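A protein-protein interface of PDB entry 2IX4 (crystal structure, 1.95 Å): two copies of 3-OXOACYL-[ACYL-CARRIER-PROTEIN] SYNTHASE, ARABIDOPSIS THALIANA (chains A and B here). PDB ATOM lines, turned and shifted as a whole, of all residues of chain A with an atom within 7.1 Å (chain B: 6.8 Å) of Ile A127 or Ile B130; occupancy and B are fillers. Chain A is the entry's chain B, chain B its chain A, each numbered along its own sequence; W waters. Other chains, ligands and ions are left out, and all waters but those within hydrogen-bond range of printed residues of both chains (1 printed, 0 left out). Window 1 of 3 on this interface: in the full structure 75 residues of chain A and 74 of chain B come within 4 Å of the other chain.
CD1 of Ile A127 touches CD1 of Ile B130 (3.8 Å). Ile A130 touches Ile B130 (CG2 to CG2, 3.6 Å). CA of Val A131 touches CB of Ala B134 (3.97 Å). CB of Ala A134 touches CB of Ala B134, at 3.6 Å. CD1 of Ile B127 touches CD1 of Ile A153 (3.97 Å). Leu A213 touches Ile B130 (CD2 to CG2, 3.9 Å). Ala B133 touches Leu A213. CD2 of Leu A213 touches CZ of Phe B149 (3.7 Å).
Ile A127 touches just one residue of chain B: Ile B130 (3.8 Å). Ile B130 touches just these residues of chain A: Ile A127 (3.8 Å), Ile A130 (3.6 Å) and Leu A213 (3.9 Å). Of the printed residues of chain A, Ala B134 touches Val A131 and Ala A134. Of the printed residues of chain B, Leu A213 touches Ile B130, Ala B133 and Phe B149. Ser A209 touches none of the printed residues of chain B. Ala A133 touches none of the printed residues of chain B. The nearest residue of chain A that does not touch Ile B130 is Val A131 (4.9 Å).
Of the 19 printed residues of chain A, 6 touch a printed residue of chain B. Hydrophobic or aromatic side chains of chain A within 4 Å of the printed part of chain B: Ile A127, Ile A130, Ala A134, Ile A153 and Leu A213. Of the 16 printed residues of chain B, 5 touch a printed residue of chain A. Hydrophobic or aromatic side chains of chain B that line the printed part of chain A: Ile B127, Ile B130, Ala B133, Ala B134 and Phe B149. Among the printed residues, 8 pairs touch across the chains.
Ile A127 touches Ile B130, but with the chains exchanged Ile A130 does not touch Ile B127 (4.4 Å). Ile B130 touches its own counterpart, Ile A130. Ala B134 touches its own counterpart, Ala A134. Ile A153 touches Ile B127, but with the chains exchanged Ile A127 does not touch Ile B153 (4.03 Å). Of the 8 pairs that touch across the chains among the printed residues, 2 have their exchanged pair printed and touching as well.
Water W1 bridges the backbone carbonyl oxygen (O) of Ile A153 (3.0 Å) and the backbone carbonyl oxygen (O) of Ile B124 (3.4 Å).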
ATOM      1  N   ILE A 124     -29.242  -3.940  13.848  1.00  0.00           N
ATOM      2  CA  ILE A 124     -28.396  -5.100  13.535  1.00  0.00           C
ATOM      3  C   ILE A 124     -28.475  -6.181  14.615  1.00  0.00           C
ATOM      4  O   ILE A 124     -28.386  -7.370  14.312  1.00  0.00           O
ATOM      5  CB  ILE A 124     -26.908  -4.711  13.319  1.00  0.00           C
ATOM      6  CG1 ILE A 124     -26.772  -3.490  12.406  1.00  0.00           C
ATOM      7  CG2 ILE A 124     -26.145  -5.872  12.708  1.00  0.00           C
ATOM      8  CD1 ILE A 124     -25.376  -2.866  12.389  1.00  0.00           C
ATOM      9  N   GLY A 125     -28.635  -5.768  15.870  1.00  0.00           N
ATOM     10  CA  GLY A 125     -28.739  -6.715  16.977  1.00  0.00           C
ATOM     11  C   GLY A 125     -27.422  -6.927  17.698  1.00  0.00           C
ATOM     12  O   GLY A 125     -26.841  -5.981  18.234  1.00  0.00           O
ATOM     13  N   SER A 126     -26.950  -8.171  17.721  1.00  0.00           N
ATOM     14  CA  SER A 126     -25.694  -8.489  18.396  1.00  0.00           C
ATOM     15  C   SER A 126     -24.764  -9.347  17.539  1.00  0.00           C
ATOM     16  O   SER A 126     -24.720 -10.572  17.684  1.00  0.00           O
ATOM     17  CB  SER A 126     -25.959  -9.149  19.751  1.00  0.00           C
ATOM     18  OG  SER A 126     -24.761  -9.238  20.497  1.00  0.00           O
ATOM     19  N   ILE A 127     -24.020  -8.688  16.652  1.00  0.00           N
ATOM     20  CA  ILE A 127     -23.048  -9.352  15.779  1.00  0.00           C
ATOM     21  C   ILE A 127     -21.963 -10.091  16.572  1.00  0.00           C
ATOM     22  O   ILE A 127     -21.570 -11.197  16.200  1.00  0.00           O
ATOM     23  CB  ILE A 127     -22.414  -8.347  14.765  1.00  0.00           C
ATOM     24  CG1 ILE A 127     -23.460  -7.849  13.757  1.00  0.00           C
ATOM     25  CG2 ILE A 127     -21.211  -8.946  14.036  1.00  0.00           C
ATOM     26  CD1 ILE A 127     -24.165  -8.940  12.957  1.00  0.00           C
ATOM     27  N   CYS A 128     -21.504  -9.489  17.669  1.00  0.00           N
ATOM     28  CA  CYS A 128     -20.415 -10.064  18.467  1.00  0.00           C
ATOM     29  C   CYS A 128     -20.752 -11.440  19.055  1.00  0.00           C
ATOM     30  O   CYS A 128     -19.881 -12.304  19.164  1.00  0.00           O
ATOM     31  CB  CYS A 128     -19.967  -9.096  19.564  1.00  0.00           C
ATOM     32  SG  CYS A 128     -21.246  -8.663  20.754  1.00  0.00           S
ATOM     33  N   ASP A 129     -22.018 -11.635  19.423  1.00  0.00           N
ATOM     34  CA  ASP A 129     -22.499 -12.920  19.927  1.00  0.00           C
ATOM     35  C   ASP A 129     -22.557 -13.978  18.825  1.00  0.00           C
ATOM     36  O   ASP A 129     -22.306 -15.159  19.080  1.00  0.00           O
ATOM     37  CB  ASP A 129     -23.871 -12.756  20.582  1.00  0.00           C
ATOM     38  CG  ASP A 129     -23.788 -12.115  21.951  1.00  0.00           C
ATOM     39  OD1 ASP A 129     -23.184 -12.721  22.861  1.00  0.00           O
ATOM     40  OD2 ASP A 129     -24.334 -11.009  22.123  1.00  0.00           O
ATOM     41  N   ILE A 130     -22.888 -13.556  17.605  1.00  0.00           N
ATOM     42  CA  ILE A 130     -22.864 -14.466  16.456  1.00  0.00           C
ATOM     43  C   ILE A 130     -21.419 -14.843  16.103  1.00  0.00           C
ATOM     44  O   ILE A 130     -21.136 -15.998  15.786  1.00  0.00           O
ATOM     45  CB  ILE A 130     -23.612 -13.890  15.219  1.00  0.00           C
ATOM     46  CG1 ILE A 130     -25.030 -13.455  15.604  1.00  0.00           C
ATOM     47  CG2 ILE A 130     -23.660 -14.935  14.092  1.00  0.00           C
ATOM     48  CD1 ILE A 130     -25.704 -12.521  14.609  1.00  0.00           C
ATOM     49  N   VAL A 131     -20.513 -13.869  16.179  1.00  0.00           N
ATOM     50  CA  VAL A 131     -19.081 -14.106  15.967  1.00  0.00           C
ATOM     51  C   VAL A 131     -18.536 -15.129  16.973  1.00  0.00           C
ATOM     52  O   VAL A 131     -17.798 -16.044  16.598  1.00  0.00           O
ATOM     53  CB  VAL A 131     -18.263 -12.778  16.014  1.00  0.00           C
ATOM     54  CG1 VAL A 131     -16.759 -13.042  16.066  1.00  0.00           C
ATOM     55  CG2 VAL A 131     -18.597 -11.900  14.814  1.00  0.00           C
ATOM     56  N   GLU A 132     -18.917 -14.977  18.241  1.00  0.00           N
ATOM     57  CA  GLU A 132     -18.472 -15.889  19.299  1.00  0.00           C
ATOM     58  C   GLU A 132     -18.980 -17.318  19.070  1.00  0.00           C
ATOM     59  O   GLU A 132     -18.244 -18.292  19.265  1.00  0.00           O
ATOM     60  CB  GLU A 132     -18.905 -15.371  20.676  1.00  0.00           C
ATOM     61  CG  GLU A 132     -18.103 -15.955  21.827  1.00  0.00           C
ATOM     62  CD  GLU A 132     -18.365 -15.279  23.169  1.00  0.00           C
ATOM     63  OE1 GLU A 132     -18.826 -14.116  23.190  1.00  0.00           O
ATOM     64  OE2 GLU A 132     -18.092 -15.919  24.211  1.00  0.00           O
ATOM     65  N   ALA A 133     -20.237 -17.429  18.649  1.00  0.00           N
ATOM     66  CA  ALA A 133     -20.855 -18.719  18.342  1.00  0.00           C
ATOM     67  C   ALA A 133     -20.225 -19.367  17.110  1.00  0.00           C
ATOM     68  O   ALA A 133     -20.004 -20.579  17.083  1.00  0.00           O
ATOM     69  CB  ALA A 133     -22.353 -18.548  18.151  1.00  0.00           C
ATOM     70  N   ALA A 134     -19.936 -18.553  16.095  1.00  0.00           N
ATOM     71  CA  ALA A 134     -19.270 -19.025  14.879  1.00  0.00           C
ATOM     72  C   ALA A 134     -17.852 -19.522  15.164  1.00  0.00           C
ATOM     73  O   ALA A 134     -17.360 -20.433  14.494  1.00  0.00           O
ATOM     74  CB  ALA A 134     -19.253 -17.934  13.824  1.00  0.00           C
ATOM     75  N   PHE A 149     -28.581 -17.889  23.072  1.00  0.00           N
ATOM     76  CA  PHE A 149     -28.029 -17.378  21.816  1.00  0.00           C
ATOM     77  C   PHE A 149     -29.087 -16.719  20.928  1.00  0.00           C
ATOM     78  O   PHE A 149     -28.938 -15.553  20.557  1.00  0.00           O
ATOM     79  CB  PHE A 149     -27.270 -18.468  21.045  1.00  0.00           C
ATOM     80  CG  PHE A 149     -26.868 -18.059  19.651  1.00  0.00           C
ATOM     81  CD1 PHE A 149     -25.936 -17.047  19.448  1.00  0.00           C
ATOM     82  CD2 PHE A 149     -27.425 -18.686  18.541  1.00  0.00           C
ATOM     83  CE1 PHE A 149     -25.570 -16.663  18.161  1.00  0.00           C
ATOM     84  CE2 PHE A 149     -27.063 -18.310  17.249  1.00  0.00           C
ATOM     85  CZ  PHE A 149     -26.133 -17.298  17.060  1.00  0.00           C
ATOM     86  N   ILE A 153     -29.814 -12.375  19.892  1.00  0.00           N
ATOM     87  CA  ILE A 153     -29.470 -11.801  18.589  1.00  0.00           C
ATOM     88  C   ILE A 153     -30.661 -11.211  17.821  1.00  0.00           C
ATOM     89  O   ILE A 153     -30.472 -10.552  16.794  1.00  0.00           O
ATOM     90  CB  ILE A 153     -28.691 -12.813  17.701  1.00  0.00           C
ATOM     91  CG1 ILE A 153     -29.583 -13.985  17.274  1.00  0.00           C
ATOM     92  CG2 ILE A 153     -27.439 -13.303  18.430  1.00  0.00           C
ATOM     93  CD1 ILE A 153     -29.031 -14.796  16.115  1.00  0.00           C
ATOM     94  N   SER A 208     -26.041  -1.409  19.653  1.00  0.00           N
ATOM     95  CA  SER A 208     -24.720  -1.595  20.225  1.00  0.00           C
ATOM     96  C   SER A 208     -23.931  -2.497  19.298  1.00  0.00           C
ATOM     97  O   SER A 208     -23.857  -3.709  19.501  1.00  0.00           O
ATOM     98  CB  SER A 208     -24.799  -2.201  21.620  1.00  0.00           C
ATOM     99  OG  SER A 208     -23.505  -2.275  22.185  1.00  0.00           O
ATOM    100  N   SER A 209     -23.358  -1.889  18.266  1.00  0.00           N
ATOM    101  CA  SER A 209     -22.649  -2.630  17.239  1.00  0.00           C
ATOM    102  C   SER A 209     -21.226  -2.092  17.036  1.00  0.00           C
ATOM    103  O   SER A 209     -20.766  -1.939  15.906  1.00  0.00           O
ATOM    104  CB  SER A 209     -23.445  -2.608  15.926  1.00  0.00           C
ATOM    105  OG  SER A 209     -23.229  -3.805  15.187  1.00  0.00           O
ATOM    106  N   ASP A 211     -17.944  -3.469  17.412  1.00  0.00           N
ATOM    107  CA  ASP A 211     -17.203  -4.709  17.566  1.00  0.00           C
ATOM    108  C   ASP A 211     -16.419  -4.991  16.290  1.00  0.00           C
ATOM    109  O   ASP A 211     -16.611  -4.315  15.272  1.00  0.00           O
ATOM    110  CB  ASP A 211     -18.144  -5.875  17.917  1.00  0.00           C
ATOM    111  CG  ASP A 211     -19.368  -5.937  17.018  1.00  0.00           C
ATOM    112  OD1 ASP A 211     -19.244  -6.373  15.853  1.00  0.00           O
ATOM    113  OD2 ASP A 211     -20.459  -5.555  17.486  1.00  0.00           O
ATOM    114  N   ALA A 212     -15.539  -5.989  16.363  1.00  0.00           N
ATOM    115  CA  ALA A 212     -14.625  -6.342  15.280  1.00  0.00           C
ATOM    116  C   ALA A 212     -15.291  -6.366  13.906  1.00  0.00           C
ATOM    117  O   ALA A 212     -14.900  -5.615  13.012  1.00  0.00           O
ATOM    118  CB  ALA A 212     -13.970  -7.674  15.570  1.00  0.00           C
ATOM    119  N   LEU A 213     -16.303  -7.221  13.756  1.00  0.00           N
ATOM    120  CA  LEU A 213     -16.921  -7.468  12.454  1.00  0.00           C
ATOM    121  C   LEU A 213     -17.761  -6.297  11.943  1.00  0.00           C
ATOM    122  O   LEU A 213     -17.802  -6.045  10.737  1.00  0.00           O
ATOM    123  CB  LEU A 213     -17.741  -8.765  12.477  1.00  0.00           C
ATOM    124  CG  LEU A 213     -18.175  -9.367  11.136  1.00  0.00           C
ATOM    125  CD1 LEU A 213     -16.977  -9.629  10.228  1.00  0.00           C
ATOM    126  CD2 LEU A 213     -18.980 -10.639  11.354  1.00  0.00           C
ATOM    127  N   SER A 214     -18.420  -5.588  12.856  1.00  0.00           N
ATOM    128  CA  SER A 214     -19.218  -4.419  12.492  1.00  0.00           C
ATOM    129  C   SER A 214     -18.326  -3.325  11.907  1.00  0.00           C
ATOM    130  O   SER A 214     -18.623  -2.771  10.842  1.00  0.00           O
ATOM    131  CB  SER A 214     -19.983  -3.883  13.703  1.00  0.00           C
ATOM    132  OG  SER A 214     -20.868  -4.856  14.234  1.00  0.00           O
ATOM    133  N   ILE B 124     -34.421 -12.880  10.975  1.00  0.00           N
ATOM    134  CA  ILE B 124     -33.022 -12.967  11.417  1.00  0.00           C
ATOM    135  C   ILE B 124     -32.020 -12.495  10.359  1.00  0.00           C
ATOM    136  O   ILE B 124     -30.943 -12.005  10.699  1.00  0.00           O
ATOM    137  CB  ILE B 124     -32.626 -14.395  11.889  1.00  0.00           C
ATOM    138  CG1 ILE B 124     -33.793 -15.093  12.595  1.00  0.00           C
ATOM    139  CG2 ILE B 124     -31.424 -14.322  12.831  1.00  0.00           C
ATOM    140  CD1 ILE B 124     -33.586 -16.591  12.832  1.00  0.00           C
ATOM    141  N   GLY B 125     -32.368 -12.646   9.085  1.00  0.00           N
ATOM    142  CA  GLY B 125     -31.498 -12.190   8.002  1.00  0.00           C
ATOM    143  C   GLY B 125     -30.656 -13.304   7.419  1.00  0.00           C
ATOM    144  O   GLY B 125     -31.189 -14.284   6.896  1.00  0.00           O
ATOM    145  N   SER B 126     -29.336 -13.158   7.512  1.00  0.00           N
ATOM    146  CA  SER B 126     -28.422 -14.136   6.929  1.00  0.00           C
ATOM    147  C   SER B 126     -27.298 -14.521   7.890  1.00  0.00           C
ATOM    148  O   SER B 126     -26.188 -13.987   7.815  1.00  0.00           O
ATOM    149  CB  SER B 126     -27.866 -13.618   5.600  1.00  0.00           C
ATOM    150  OG  SER B 126     -27.200 -14.651   4.895  1.00  0.00           O
ATOM    151  N   ILE B 127     -27.600 -15.453   8.792  1.00  0.00           N
ATOM    152  CA  ILE B 127     -26.624 -15.960   9.758  1.00  0.00           C
ATOM    153  C   ILE B 127     -25.421 -16.624   9.078  1.00  0.00           C
ATOM    154  O   ILE B 127     -24.291 -16.469   9.539  1.00  0.00           O
ATOM    155  CB  ILE B 127     -27.271 -16.928  10.794  1.00  0.00           C
ATOM    156  CG1 ILE B 127     -28.309 -16.184  11.646  1.00  0.00           C
ATOM    157  CG2 ILE B 127     -26.205 -17.562  11.691  1.00  0.00           C
ATOM    158  CD1 ILE B 127     -28.888 -16.991  12.810  1.00  0.00           C
ATOM    159  N   CYS B 128     -25.665 -17.346   7.983  1.00  0.00           N
ATOM    160  CA  CYS B 128     -24.598 -18.055   7.271  1.00  0.00           C
ATOM    161  C   CYS B 128     -23.543 -17.105   6.702  1.00  0.00           C
ATOM    162  O   CYS B 128     -22.357 -17.442   6.653  1.00  0.00           O
ATOM    163  CB  CYS B 128     -25.168 -18.957   6.169  1.00  0.00           C
ATOM    164  SG  CYS B 128     -26.005 -18.087   4.826  1.00  0.00           S
ATOM    165  N   ASP B 129     -23.979 -15.920   6.276  1.00  0.00           N
ATOM    166  CA  ASP B 129     -23.067 -14.882   5.802  1.00  0.00           C
ATOM    167  C   ASP B 129     -22.223 -14.300   6.933  1.00  0.00           C
ATOM    168  O   ASP B 129     -21.048 -13.989   6.734  1.00  0.00           O
ATOM    169  CB  ASP B 129     -23.837 -13.773   5.086  1.00  0.00           C
ATOM    170  CG  ASP B 129     -24.225 -14.155   3.671  1.00  0.00           C
ATOM    171  OD1 ASP B 129     -23.356 -14.653   2.921  1.00  0.00           O
ATOM    172  OD2 ASP B 129     -25.397 -13.948   3.300  1.00  0.00           O
ATOM    173  N   ILE B 130     -22.823 -14.154   8.115  1.00  0.00           N
ATOM    174  CA  ILE B 130     -22.091 -13.675   9.290  1.00  0.00           C
ATOM    175  C   ILE B 130     -21.095 -14.731   9.780  1.00  0.00           C
ATOM    176  O   ILE B 130     -20.011 -14.394  10.254  1.00  0.00           O
ATOM    177  CB  ILE B 130     -23.042 -13.231  10.434  1.00  0.00           C
ATOM    178  CG1 ILE B 130     -24.027 -12.173   9.923  1.00  0.00           C
ATOM    179  CG2 ILE B 130     -22.245 -12.682  11.631  1.00  0.00           C
ATOM    180  CD1 ILE B 130     -25.214 -11.914  10.843  1.00  0.00           C
ATOM    181  N   VAL B 131     -21.469 -16.004   9.652  1.00  0.00           N
ATOM    182  CA  VAL B 131     -20.589 -17.121  10.011  1.00  0.00           C
ATOM    183  C   VAL B 131     -19.344 -17.154   9.112  1.00  0.00           C
ATOM    184  O   VAL B 131     -18.220 -17.321   9.601  1.00  0.00           O
ATOM    185  CB  VAL B 131     -21.350 -18.484   9.985  1.00  0.00           C
ATOM    186  CG1 VAL B 131     -20.384 -19.665   9.991  1.00  0.00           C
ATOM    187  CG2 VAL B 131     -22.302 -18.580  11.173  1.00  0.00           C
ATOM    188  N   GLU B 132     -19.552 -16.978   7.809  1.00  0.00           N
ATOM    189  CA  GLU B 132     -18.446 -16.921   6.846  1.00  0.00           C
ATOM    190  C   GLU B 132     -17.479 -15.776   7.153  1.00  0.00           C
ATOM    191  O   GLU B 132     -16.261 -15.946   7.079  1.00  0.00           O
ATOM    192  CB  GLU B 132     -18.968 -16.809   5.410  1.00  0.00           C
ATOM    193  CG  GLU B 132     -19.564 -18.098   4.867  1.00  0.00           C
ATOM    194  CD  GLU B 132     -19.671 -18.134   3.342  1.00  0.00           C
ATOM    195  OE1 GLU B 132     -19.344 -17.125   2.677  1.00  0.00           O
ATOM    196  OE2 GLU B 132     -20.088 -19.186   2.809  1.00  0.00           O
ATOM    197  N   ALA B 133     -18.034 -14.617   7.504  1.00  0.00           N
ATOM    198  CA  ALA B 133     -17.237 -13.445   7.867  1.00  0.00           C
ATOM    199  C   ALA B 133     -16.469 -13.651   9.178  1.00  0.00           C
ATOM    200  O   ALA B 133     -15.304 -13.268   9.288  1.00  0.00           O
ATOM    201  CB  ALA B 133     -18.124 -12.216   7.952  1.00  0.00           C
ATOM    202  N   ALA B 134     -17.127 -14.267  10.160  1.00  0.00           N
ATOM    203  CA  ALA B 134     -16.502 -14.560  11.451  1.00  0.00           C
ATOM    204  C   ALA B 134     -15.356 -15.562  11.314  1.00  0.00           C
ATOM    205  O   ALA B 134     -14.379 -15.509  12.070  1.00  0.00           O
ATOM    206  CB  ALA B 134     -17.538 -15.062  12.437  1.00  0.00           C
ATOM    207  N   GLN B 135     -15.477 -16.463  10.339  1.00  0.00           N
ATOM    208  CA  GLN B 135     -14.412 -17.419  10.012  1.00  0.00           C
ATOM    209  C   GLN B 135     -13.145 -16.699   9.544  1.00  0.00           C
ATOM    210  O   GLN B 135     -12.032 -17.146   9.827  1.00  0.00           O
ATOM    211  CB  GLN B 135     -14.891 -18.410   8.943  1.00  0.00           C
ATOM    212  CG  GLN B 135     -13.942 -19.571   8.674  1.00  0.00           C
ATOM    213  CD  GLN B 135     -14.280 -20.332   7.403  1.00  0.00           C
ATOM    214  OE1 GLN B 135     -15.176 -19.946   6.650  1.00  0.00           O
ATOM    215  NE2 GLN B 135     -13.559 -21.419   7.157  1.00  0.00           N
ATOM    216  N   PHE B 149     -20.988  -7.182   2.474  1.00  0.00           N
ATOM    217  CA  PHE B 149     -21.321  -7.923   3.690  1.00  0.00           C
ATOM    218  C   PHE B 149     -22.463  -7.281   4.476  1.00  0.00           C
ATOM    219  O   PHE B 149     -23.458  -7.945   4.771  1.00  0.00           O
ATOM    220  CB  PHE B 149     -20.087  -8.126   4.584  1.00  0.00           C
ATOM    221  CG  PHE B 149     -20.417  -8.624   5.971  1.00  0.00           C
ATOM    222  CD1 PHE B 149     -20.880  -9.924   6.170  1.00  0.00           C
ATOM    223  CD2 PHE B 149     -20.270  -7.789   7.076  1.00  0.00           C
ATOM    224  CE1 PHE B 149     -21.196 -10.382   7.451  1.00  0.00           C
ATOM    225  CE2 PHE B 149     -20.581  -8.241   8.360  1.00  0.00           C
ATOM    226  CZ  PHE B 149     -21.043  -9.541   8.544  1.00  0.00           C
ATOM    227  N   ILE B 150     -22.315  -5.998   4.812  1.00  0.00           N
ATOM    228  CA  ILE B 150     -23.335  -5.276   5.584  1.00  0.00           C
ATOM    229  C   ILE B 150     -24.698  -5.221   4.865  1.00  0.00           C
ATOM    230  O   ILE B 150     -25.714  -5.585   5.463  1.00  0.00           O
ATOM    231  CB  ILE B 150     -22.855  -3.854   6.034  1.00  0.00           C
ATOM    232  CG1 ILE B 150     -21.708  -3.955   7.055  1.00  0.00           C
ATOM    233  CG2 ILE B 150     -24.015  -3.018   6.586  1.00  0.00           C
ATOM    234  CD1 ILE B 150     -22.094  -4.543   8.421  1.00  0.00           C
ATOM    235  N   LYS B 152     -26.059  -7.194   2.746  1.00  0.00           N
ATOM    236  CA  LYS B 152     -26.745  -8.487   2.594  1.00  0.00           C
ATOM    237  C   LYS B 152     -27.193  -9.164   3.898  1.00  0.00           C
ATOM    238  O   LYS B 152     -27.877 -10.185   3.857  1.00  0.00           O
ATOM    239  CB  LYS B 152     -25.961  -9.454   1.686  1.00  0.00           C
ATOM    240  CG  LYS B 152     -24.688 -10.048   2.256  1.00  0.00           C
ATOM    241  CD  LYS B 152     -24.128 -11.094   1.289  1.00  0.00           C
ATOM    242  CE  LYS B 152     -22.604 -11.056   1.210  1.00  0.00           C
ATOM    243  NZ  LYS B 152     -21.904 -11.609   2.418  1.00  0.00           N
ATOM    244  N   ILE B 153     -26.833  -8.589   5.044  1.00  0.00           N
ATOM    245  CA  ILE B 153     -27.253  -9.146   6.337  1.00  0.00           C
ATOM    246  C   ILE B 153     -28.358  -8.344   7.038  1.00  0.00           C
ATOM    247  O   ILE B 153     -28.923  -8.801   8.032  1.00  0.00           O
ATOM    248  CB  ILE B 153     -26.053  -9.381   7.309  1.00  0.00           C
ATOM    249  CG1 ILE B 153     -25.408  -8.055   7.734  1.00  0.00           C
ATOM    250  CG2 ILE B 153     -25.039 -10.341   6.687  1.00  0.00           C
ATOM    251  CD1 ILE B 153     -24.636  -8.122   9.042  1.00  0.00           C
HETATM  252  O   HOH W   1     -30.536 -10.805  13.806  1.00  0.00           O
